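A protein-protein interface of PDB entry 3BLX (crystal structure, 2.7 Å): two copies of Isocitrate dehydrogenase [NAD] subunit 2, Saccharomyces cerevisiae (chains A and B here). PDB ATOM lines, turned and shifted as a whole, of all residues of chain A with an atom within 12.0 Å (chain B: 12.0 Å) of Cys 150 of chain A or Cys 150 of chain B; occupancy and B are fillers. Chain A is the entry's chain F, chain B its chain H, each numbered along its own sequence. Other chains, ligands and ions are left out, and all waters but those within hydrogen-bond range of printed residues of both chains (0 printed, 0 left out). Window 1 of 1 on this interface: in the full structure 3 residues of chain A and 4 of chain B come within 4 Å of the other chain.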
ATOM      1  N   GLU A 146       7.592  10.777   4.951  1.00  0.00           N
ATOM      2  CA  GLU A 146       7.375   9.785   3.905  1.00  0.00           C
ATOM      3  C   GLU A 146       7.072  10.407   2.537  1.00  0.00           C
ATOM      4  O   GLU A 146       6.393  11.427   2.442  1.00  0.00           O
ATOM      5  CB  GLU A 146       6.213   8.897   4.278  1.00  0.00           C
ATOM      6  CG  GLU A 146       6.468   7.983   5.445  1.00  0.00           C
ATOM      7  CD  GLU A 146       5.342   6.957   5.628  1.00  0.00           C
ATOM      8  OE1 GLU A 146       5.629   5.735   5.545  1.00  0.00           O
ATOM      9  OE2 GLU A 146       4.170   7.370   5.839  1.00  0.00           O
ATOM     10  N   HIS A 147       7.553   9.786   1.472  1.00  0.00           N
ATOM     11  CA  HIS A 147       7.155  10.216   0.138  1.00  0.00           C
ATOM     12  C   HIS A 147       7.299   9.133  -0.880  1.00  0.00           C
ATOM     13  O   HIS A 147       8.020   8.160  -0.678  1.00  0.00           O
ATOM     14  CB  HIS A 147       7.935  11.448  -0.315  1.00  0.00           C
ATOM     15  CG  HIS A 147       9.358  11.175  -0.674  1.00  0.00           C
ATOM     16  ND1 HIS A 147       9.925  11.636  -1.844  1.00  0.00           N
ATOM     17  CD2 HIS A 147      10.338  10.522  -0.010  1.00  0.00           C
ATOM     18  CE1 HIS A 147      11.202  11.282  -1.875  1.00  0.00           C
ATOM     19  NE2 HIS A 147      11.476  10.603  -0.775  1.00  0.00           N
ATOM     20  N   ILE A 148       6.608   9.317  -1.989  1.00  0.00           N
ATOM     21  CA  ILE A 148       6.642   8.368  -3.076  1.00  0.00           C
ATOM     22  C   ILE A 148       7.765   8.714  -4.005  1.00  0.00           C
ATOM     23  O   ILE A 148       7.795   9.832  -4.541  1.00  0.00           O
ATOM     24  CB  ILE A 148       5.336   8.422  -3.827  1.00  0.00           C
ATOM     25  CG1 ILE A 148       4.199   8.160  -2.844  1.00  0.00           C
ATOM     26  CG2 ILE A 148       5.325   7.382  -4.943  1.00  0.00           C
ATOM     27  CD1 ILE A 148       2.880   7.986  -3.503  1.00  0.00           C
ATOM     28  N   VAL A 149       8.691   7.772  -4.179  1.00  0.00           N
ATOM     29  CA  VAL A 149       9.850   8.051  -5.005  1.00  0.00           C
ATOM     30  C   VAL A 149       9.542   7.714  -6.455  1.00  0.00           C
ATOM     31  O   VAL A 149       9.491   8.607  -7.296  1.00  0.00           O
ATOM     32  CB  VAL A 149      11.071   7.298  -4.510  1.00  0.00           C
ATOM     33  CG1 VAL A 149      12.273   7.597  -5.419  1.00  0.00           C
ATOM     34  CG2 VAL A 149      11.374   7.724  -3.120  1.00  0.00           C
ATOM     35  N   CYS A 150       9.383   6.423  -6.742  1.00  0.00           N
ATOM     36  CA  CYS A 150       8.898   5.984  -8.040  1.00  0.00           C
ATOM     37  C   CYS A 150       7.499   5.478  -7.746  1.00  0.00           C
ATOM     38  O   CYS A 150       7.080   5.499  -6.604  1.00  0.00           O
ATOM     39  CB  CYS A 150       9.780   4.896  -8.689  1.00  0.00           C
ATOM     40  SG  CYS A 150      11.293   4.513  -7.876  1.00  0.00           S
ATOM     41  N   PRO A 151       6.774   5.030  -8.779  1.00  0.00           N
ATOM     42  CA  PRO A 151       5.324   4.787  -8.688  1.00  0.00           C
ATOM     43  C   PRO A 151       4.813   3.802  -7.630  1.00  0.00           C
ATOM     44  O   PRO A 151       3.721   4.051  -7.105  1.00  0.00           O
ATOM     45  CB  PRO A 151       4.955   4.314 -10.091  1.00  0.00           C
ATOM     46  CG  PRO A 151       6.001   4.953 -10.980  1.00  0.00           C
ATOM     47  CD  PRO A 151       7.264   4.943 -10.170  1.00  0.00           C
ATOM     48  N   GLY A 152       5.521   2.723  -7.311  1.00  0.00           N
ATOM     49  CA  GLY A 152       5.029   1.874  -6.222  1.00  0.00           C
ATOM     50  C   GLY A 152       5.923   1.843  -4.981  1.00  0.00           C
ATOM     51  O   GLY A 152       6.007   0.834  -4.290  1.00  0.00           O
ATOM     52  N   VAL A 153       6.589   2.952  -4.687  1.00  0.00           N
ATOM     53  CA  VAL A 153       7.711   2.889  -3.796  1.00  0.00           C
ATOM     54  C   VAL A 153       7.664   4.030  -2.808  1.00  0.00           C
ATOM     55  O   VAL A 153       7.864   5.185  -3.177  1.00  0.00           O
ATOM     56  CB  VAL A 153       9.036   2.978  -4.563  1.00  0.00           C
ATOM     57  CG1 VAL A 153      10.191   2.928  -3.576  1.00  0.00           C
ATOM     58  CG2 VAL A 153       9.141   1.869  -5.609  1.00  0.00           C
ATOM     59  N   VAL A 154       7.414   3.697  -1.546  1.00  0.00           N
ATOM     60  CA  VAL A 154       7.462   4.680  -0.476  1.00  0.00           C
ATOM     61  C   VAL A 154       8.800   4.704   0.233  1.00  0.00           C
ATOM     62  O   VAL A 154       9.274   3.676   0.704  1.00  0.00           O
ATOM     63  CB  VAL A 154       6.406   4.403   0.590  1.00  0.00           C
ATOM     64  CG1 VAL A 154       6.393   5.541   1.564  1.00  0.00           C
ATOM     65  CG2 VAL A 154       5.030   4.240  -0.029  1.00  0.00           C
ATOM     66  N   GLN A 155       9.399   5.883   0.317  1.00  0.00           N
ATOM     67  CA  GLN A 155      10.649   6.052   1.037  1.00  0.00           C
ATOM     68  C   GLN A 155      10.357   6.775   2.377  1.00  0.00           C
ATOM     69  O   GLN A 155       9.552   7.686   2.435  1.00  0.00           O
ATOM     70  CB  GLN A 155      11.655   6.813   0.169  1.00  0.00           C
ATOM     71  CG  GLN A 155      13.048   6.868   0.728  1.00  0.00           C
ATOM     72  CD  GLN A 155      13.975   7.721  -0.106  1.00  0.00           C
ATOM     73  OE1 GLN A 155      13.582   8.755  -0.626  1.00  0.00           O
ATOM     74  NE2 GLN A 155      15.202   7.297  -0.231  1.00  0.00           N
ATOM     75  N   SER A 156      10.990   6.330   3.459  1.00  0.00           N
ATOM     76  CA  SER A 156      10.863   6.963   4.774  1.00  0.00           C
ATOM     77  C   SER A 156      12.161   7.630   5.127  1.00  0.00           C
ATOM     78  O   SER A 156      13.248   7.095   4.854  1.00  0.00           O
ATOM     79  CB  SER A 156      10.564   5.906   5.832  1.00  0.00           C
ATOM     80  OG  SER A 156       9.372   5.200   5.534  1.00  0.00           O
ATOM     81  N   ILE A 157      12.068   8.805   5.736  1.00  0.00           N
ATOM     82  CA  ILE A 157      13.270   9.510   6.194  1.00  0.00           C
ATOM     83  C   ILE A 157      13.128   9.736   7.703  1.00  0.00           C
ATOM     84  O   ILE A 157      12.106  10.214   8.150  1.00  0.00           O
ATOM     85  CB  ILE A 157      13.464  10.827   5.425  1.00  0.00           C
ATOM     86  CG1 ILE A 157      13.343  10.559   3.926  1.00  0.00           C
ATOM     87  CG2 ILE A 157      14.794  11.427   5.720  1.00  0.00           C
ATOM     88  CD1 ILE A 157      13.362  11.798   3.097  1.00  0.00           C
ATOM     89  N   GLU B 146      24.710   9.539  -3.808  1.00  0.00           N
ATOM     90  CA  GLU B 146      23.832   8.941  -4.809  1.00  0.00           C
ATOM     91  C   GLU B 146      23.545   7.493  -4.483  1.00  0.00           C
ATOM     92  O   GLU B 146      24.418   6.766  -4.025  1.00  0.00           O
ATOM     93  CB  GLU B 146      24.463   9.013  -6.189  1.00  0.00           C
ATOM     94  CG  GLU B 146      24.449  10.381  -6.812  1.00  0.00           C
ATOM     95  CD  GLU B 146      24.866  10.345  -8.272  1.00  0.00           C
ATOM     96  OE1 GLU B 146      24.079  10.805  -9.139  1.00  0.00           O
ATOM     97  OE2 GLU B 146      25.979   9.847  -8.545  1.00  0.00           O
ATOM     98  N   HIS B 147      22.320   7.055  -4.726  1.00  0.00           N
ATOM     99  CA  HIS B 147      22.058   5.629  -4.600  1.00  0.00           C
ATOM    100  C   HIS B 147      20.900   5.171  -5.462  1.00  0.00           C
ATOM    101  O   HIS B 147      20.069   5.976  -5.901  1.00  0.00           O
ATOM    102  CB  HIS B 147      21.864   5.234  -3.123  1.00  0.00           C
ATOM    103  CG  HIS B 147      20.557   5.673  -2.536  1.00  0.00           C
ATOM    104  ND1 HIS B 147      19.734   4.818  -1.832  1.00  0.00           N
ATOM    105  CD2 HIS B 147      19.931   6.872  -2.544  1.00  0.00           C
ATOM    106  CE1 HIS B 147      18.652   5.471  -1.441  1.00  0.00           C
ATOM    107  NE2 HIS B 147      18.748   6.720  -1.858  1.00  0.00           N
ATOM    108  N   ILE B 148      20.853   3.872  -5.711  1.00  0.00           N
ATOM    109  CA  ILE B 148      19.760   3.297  -6.465  1.00  0.00           C
ATOM    110  C   ILE B 148      18.575   2.934  -5.559  1.00  0.00           C
ATOM    111  O   ILE B 148      18.705   2.094  -4.670  1.00  0.00           O
ATOM    112  CB  ILE B 148      20.253   2.072  -7.227  1.00  0.00           C
ATOM    113  CG1 ILE B 148      21.423   2.448  -8.123  1.00  0.00           C
ATOM    114  CG2 ILE B 148      19.144   1.500  -8.083  1.00  0.00           C
ATOM    115  CD1 ILE B 148      22.088   1.245  -8.776  1.00  0.00           C
ATOM    116  N   VAL B 149      17.423   3.565  -5.777  1.00  0.00           N
ATOM    117  CA  VAL B 149      16.267   3.302  -4.928  1.00  0.00           C
ATOM    118  C   VAL B 149      15.461   2.089  -5.396  1.00  0.00           C
ATOM    119  O   VAL B 149      15.392   1.075  -4.697  1.00  0.00           O
ATOM    120  CB  VAL B 149      15.367   4.510  -4.808  1.00  0.00           C
ATOM    121  CG1 VAL B 149      14.273   4.226  -3.800  1.00  0.00           C
ATOM    122  CG2 VAL B 149      16.167   5.655  -4.341  1.00  0.00           C
ATOM    123  N   CYS B 150      14.827   2.199  -6.557  1.00  0.00           N
ATOM    124  CA  CYS B 150      14.302   1.008  -7.222  1.00  0.00           C
ATOM    125  C   CYS B 150      15.160   0.744  -8.456  1.00  0.00           C
ATOM    126  O   CYS B 150      16.086   1.503  -8.748  1.00  0.00           O
ATOM    127  CB  CYS B 150      12.805   1.124  -7.539  1.00  0.00           C
ATOM    128  SG  CYS B 150      12.085   2.738  -7.316  1.00  0.00           S
ATOM    129  N   PRO B 151      14.876  -0.342  -9.171  1.00  0.00           N
ATOM    130  CA  PRO B 151      15.817  -0.846 -10.178  1.00  0.00           C
ATOM    131  C   PRO B 151      16.326   0.146 -11.236  1.00  0.00           C
ATOM    132  O   PRO B 151      17.490   0.029 -11.610  1.00  0.00           O
ATOM    133  CB  PRO B 151      15.043  -1.992 -10.827  1.00  0.00           C
ATOM    134  CG  PRO B 151      14.110  -2.456  -9.738  1.00  0.00           C
ATOM    135  CD  PRO B 151      13.703  -1.220  -9.017  1.00  0.00           C
ATOM    136  N   GLY B 152      15.528   1.084 -11.729  1.00  0.00           N
ATOM    137  CA  GLY B 152      16.099   2.015 -12.698  1.00  0.00           C
ATOM    138  C   GLY B 152      16.136   3.459 -12.236  1.00  0.00           C
ATOM    139  O   GLY B 152      16.003   4.391 -13.035  1.00  0.00           O
ATOM    140  N   VAL B 153      16.308   3.648 -10.936  1.00  0.00           N
ATOM    141  CA  VAL B 153      16.060   4.948 -10.344  1.00  0.00           C
ATOM    142  C   VAL B 153      17.200   5.361  -9.468  1.00  0.00           C
ATOM    143  O   VAL B 153      17.492   4.702  -8.483  1.00  0.00           O
ATOM    144  CB  VAL B 153      14.798   4.932  -9.538  1.00  0.00           C
ATOM    145  CG1 VAL B 153      14.521   6.357  -8.999  1.00  0.00           C
ATOM    146  CG2 VAL B 153      13.680   4.394 -10.391  1.00  0.00           C
ATOM    147  N   VAL B 154      17.872   6.437  -9.844  1.00  0.00           N
ATOM    148  CA  VAL B 154      18.907   7.029  -8.996  1.00  0.00           C
ATOM    149  C   VAL B 154      18.379   8.209  -8.190  1.00  0.00           C
ATOM    150  O   VAL B 154      17.756   9.129  -8.705  1.00  0.00           O
ATOM    151  CB  VAL B 154      20.064   7.530  -9.825  1.00  0.00           C
ATOM    152  CG1 VAL B 154      21.148   8.055  -8.923  1.00  0.00           C
ATOM    153  CG2 VAL B 154      20.593   6.411 -10.708  1.00  0.00           C
ATOM    154  N   GLN B 155      18.608   8.181  -6.900  1.00  0.00           N
ATOM    155  CA  GLN B 155      18.211   9.315  -6.080  1.00  0.00           C
ATOM    156  C   GLN B 155      19.459  10.082  -5.620  1.00  0.00           C
ATOM    157  O   GLN B 155      20.446   9.488  -5.230  1.00  0.00           O
ATOM    158  CB  GLN B 155      17.369   8.834  -4.907  1.00  0.00           C
ATOM    159  CG  GLN B 155      16.908   9.944  -4.047  1.00  0.00           C
ATOM    160  CD  GLN B 155      16.160   9.442  -2.865  1.00  0.00           C
ATOM    161  OE1 GLN B 155      16.603   8.529  -2.186  1.00  0.00           O
ATOM    162  NE2 GLN B 155      15.017  10.056  -2.590  1.00  0.00           N
ATOM    163  N   SER B 156      19.432  11.403  -5.713  1.00  0.00           N
ATOM    164  CA  SER B 156      20.557  12.221  -5.246  1.00  0.00           C
ATOM    165  C   SER B 156      20.182  12.871  -3.929  1.00  0.00           C
ATOM    166  O   SER B 156      19.032  13.260  -3.726  1.00  0.00           O
ATOM    167  CB  SER B 156      20.895  13.311  -6.254  1.00  0.00           C
ATOM    168  OG  SER B 156      21.273  12.731  -7.487  1.00  0.00           O
ATOM    169  N   ILE B 157      21.148  12.973  -3.028  1.00  0.00           N
ATOM    170  CA  ILE B 157      20.917  13.636  -1.763  1.00  0.00           C
ATOM    171  C   ILE B 157      21.968  14.722  -1.612  1.00  0.00           C
ATOM    172  O   ILE B 157      23.150  14.460  -1.728  1.00  0.00           O
ATOM    173  CB  ILE B 157      20.960  12.633  -0.613  1.00  0.00           C
ATOM    174  CG1 ILE B 157      20.037  11.454  -0.936  1.00  0.00           C
ATOM    175  CG2 ILE B 157      20.575  13.303   0.709  1.00  0.00           C
ATOM    176  CD1 ILE B 157      20.198  10.300   0.001  1.00  0.00           C
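A ring nitrogen (NE2) of His 147 of chain B lies within hydrogen-bond range of the side-chain amide oxygen (OE1) of Gln 155 of chain B. NE2 of His 147 of chain A sits at hydrogen-bond distance from OE1 of Gln 155 of chain A, at 2.8 Å.
Among the printed residues, pairs that only touch across the chains: Cys 150 of chain A with Val 153 of chain B, Val 153 of chain A with Cys 150 of chain B and Gln 155 of chain A with His 147 of chain B.
Cys 150 of chain A touches its own counterpart, Cys 150 of chain B. Cys 150 of chain A touches Val 153 of chain B, and with the chains exchanged Val 153 of chain A touches Cys 150 of chain B. Gln 155 of chain A touches His 147 of chain B, but with the chains exchanged His 147 of chain A does not touch Gln 155 of chain B (4.02 Å). Gln 155 of chain A touches its own counterpart, Gln 155 of chain B. Positions printed for both chains: 146, 147, 148, 149, 150, 151, 152, 153, 154, 155, 156 and 157. Of the 5 pairs that touch across the chains among the printed residues, 4 have their exchanged pair printed and touching as well.
The side-chain sulfur (SG) of Cys 150 of chain A is disulfide-bonded to the side-chain sulfur (SG) of Cys 150 of chain B (2.0 Å). The side-chain amide oxygen (OE1) of Gln 155 of chain B lies within hydrogen-bond range of the side-chain amide nitrogen (NE2) of Gln 155 of chain A, 2.7 Å away.
Cys 150 of chain A touches just these residues of chain B: Cys 150 and Val 153. No residue of chain B comes within 4 Å of Gly 152 of chain A. Of chain B, only Cys 150 comes within 4 Å of Val 153 of chain A. Of the printed residues of chain B, Gln 155 of chain A touches His 147 (3.9 Å) and Gln 155 (2.7 Å). Printed residues of chain A within 4 Å of His 147 of chain B: Gln 155. No residue of chain A comes within 4 Å of Val 149 of chain B. Cys 150 of chain B touches two residues of chain A. No residue of chain A comes within 4 Å of Pro 151 of chain B. Val 153 of chain B touches just one residue of chain A: Cys 150. Val 154 of chain B touches none of the printed residues of chain A. Printed residues of chain A within 4 Å of Gln 155 of chain B: Gln 155. The nearest residue of chain A that does not touch Cys 150 of chain B is Val 149 of chain A (5.2 Å).
Of the 12 printed residues of chain B, 4 touch a printed residue of chain A. Printed residues of chain B that touch a printed residue of chain A: His 147, Cys 150, Val 153 and Gln 155. Hydrophobic or aromatic side chains of chain B that line the printed part of chain A: His 147 and Val 153. Of the 12 printed residues of chain A, 3 touch a printed residue of chain B. Among the printed residues, no Asp or Glu carboxylate lies within 4 Å of a Lys or Arg side-chain nitrogen of the other chain.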
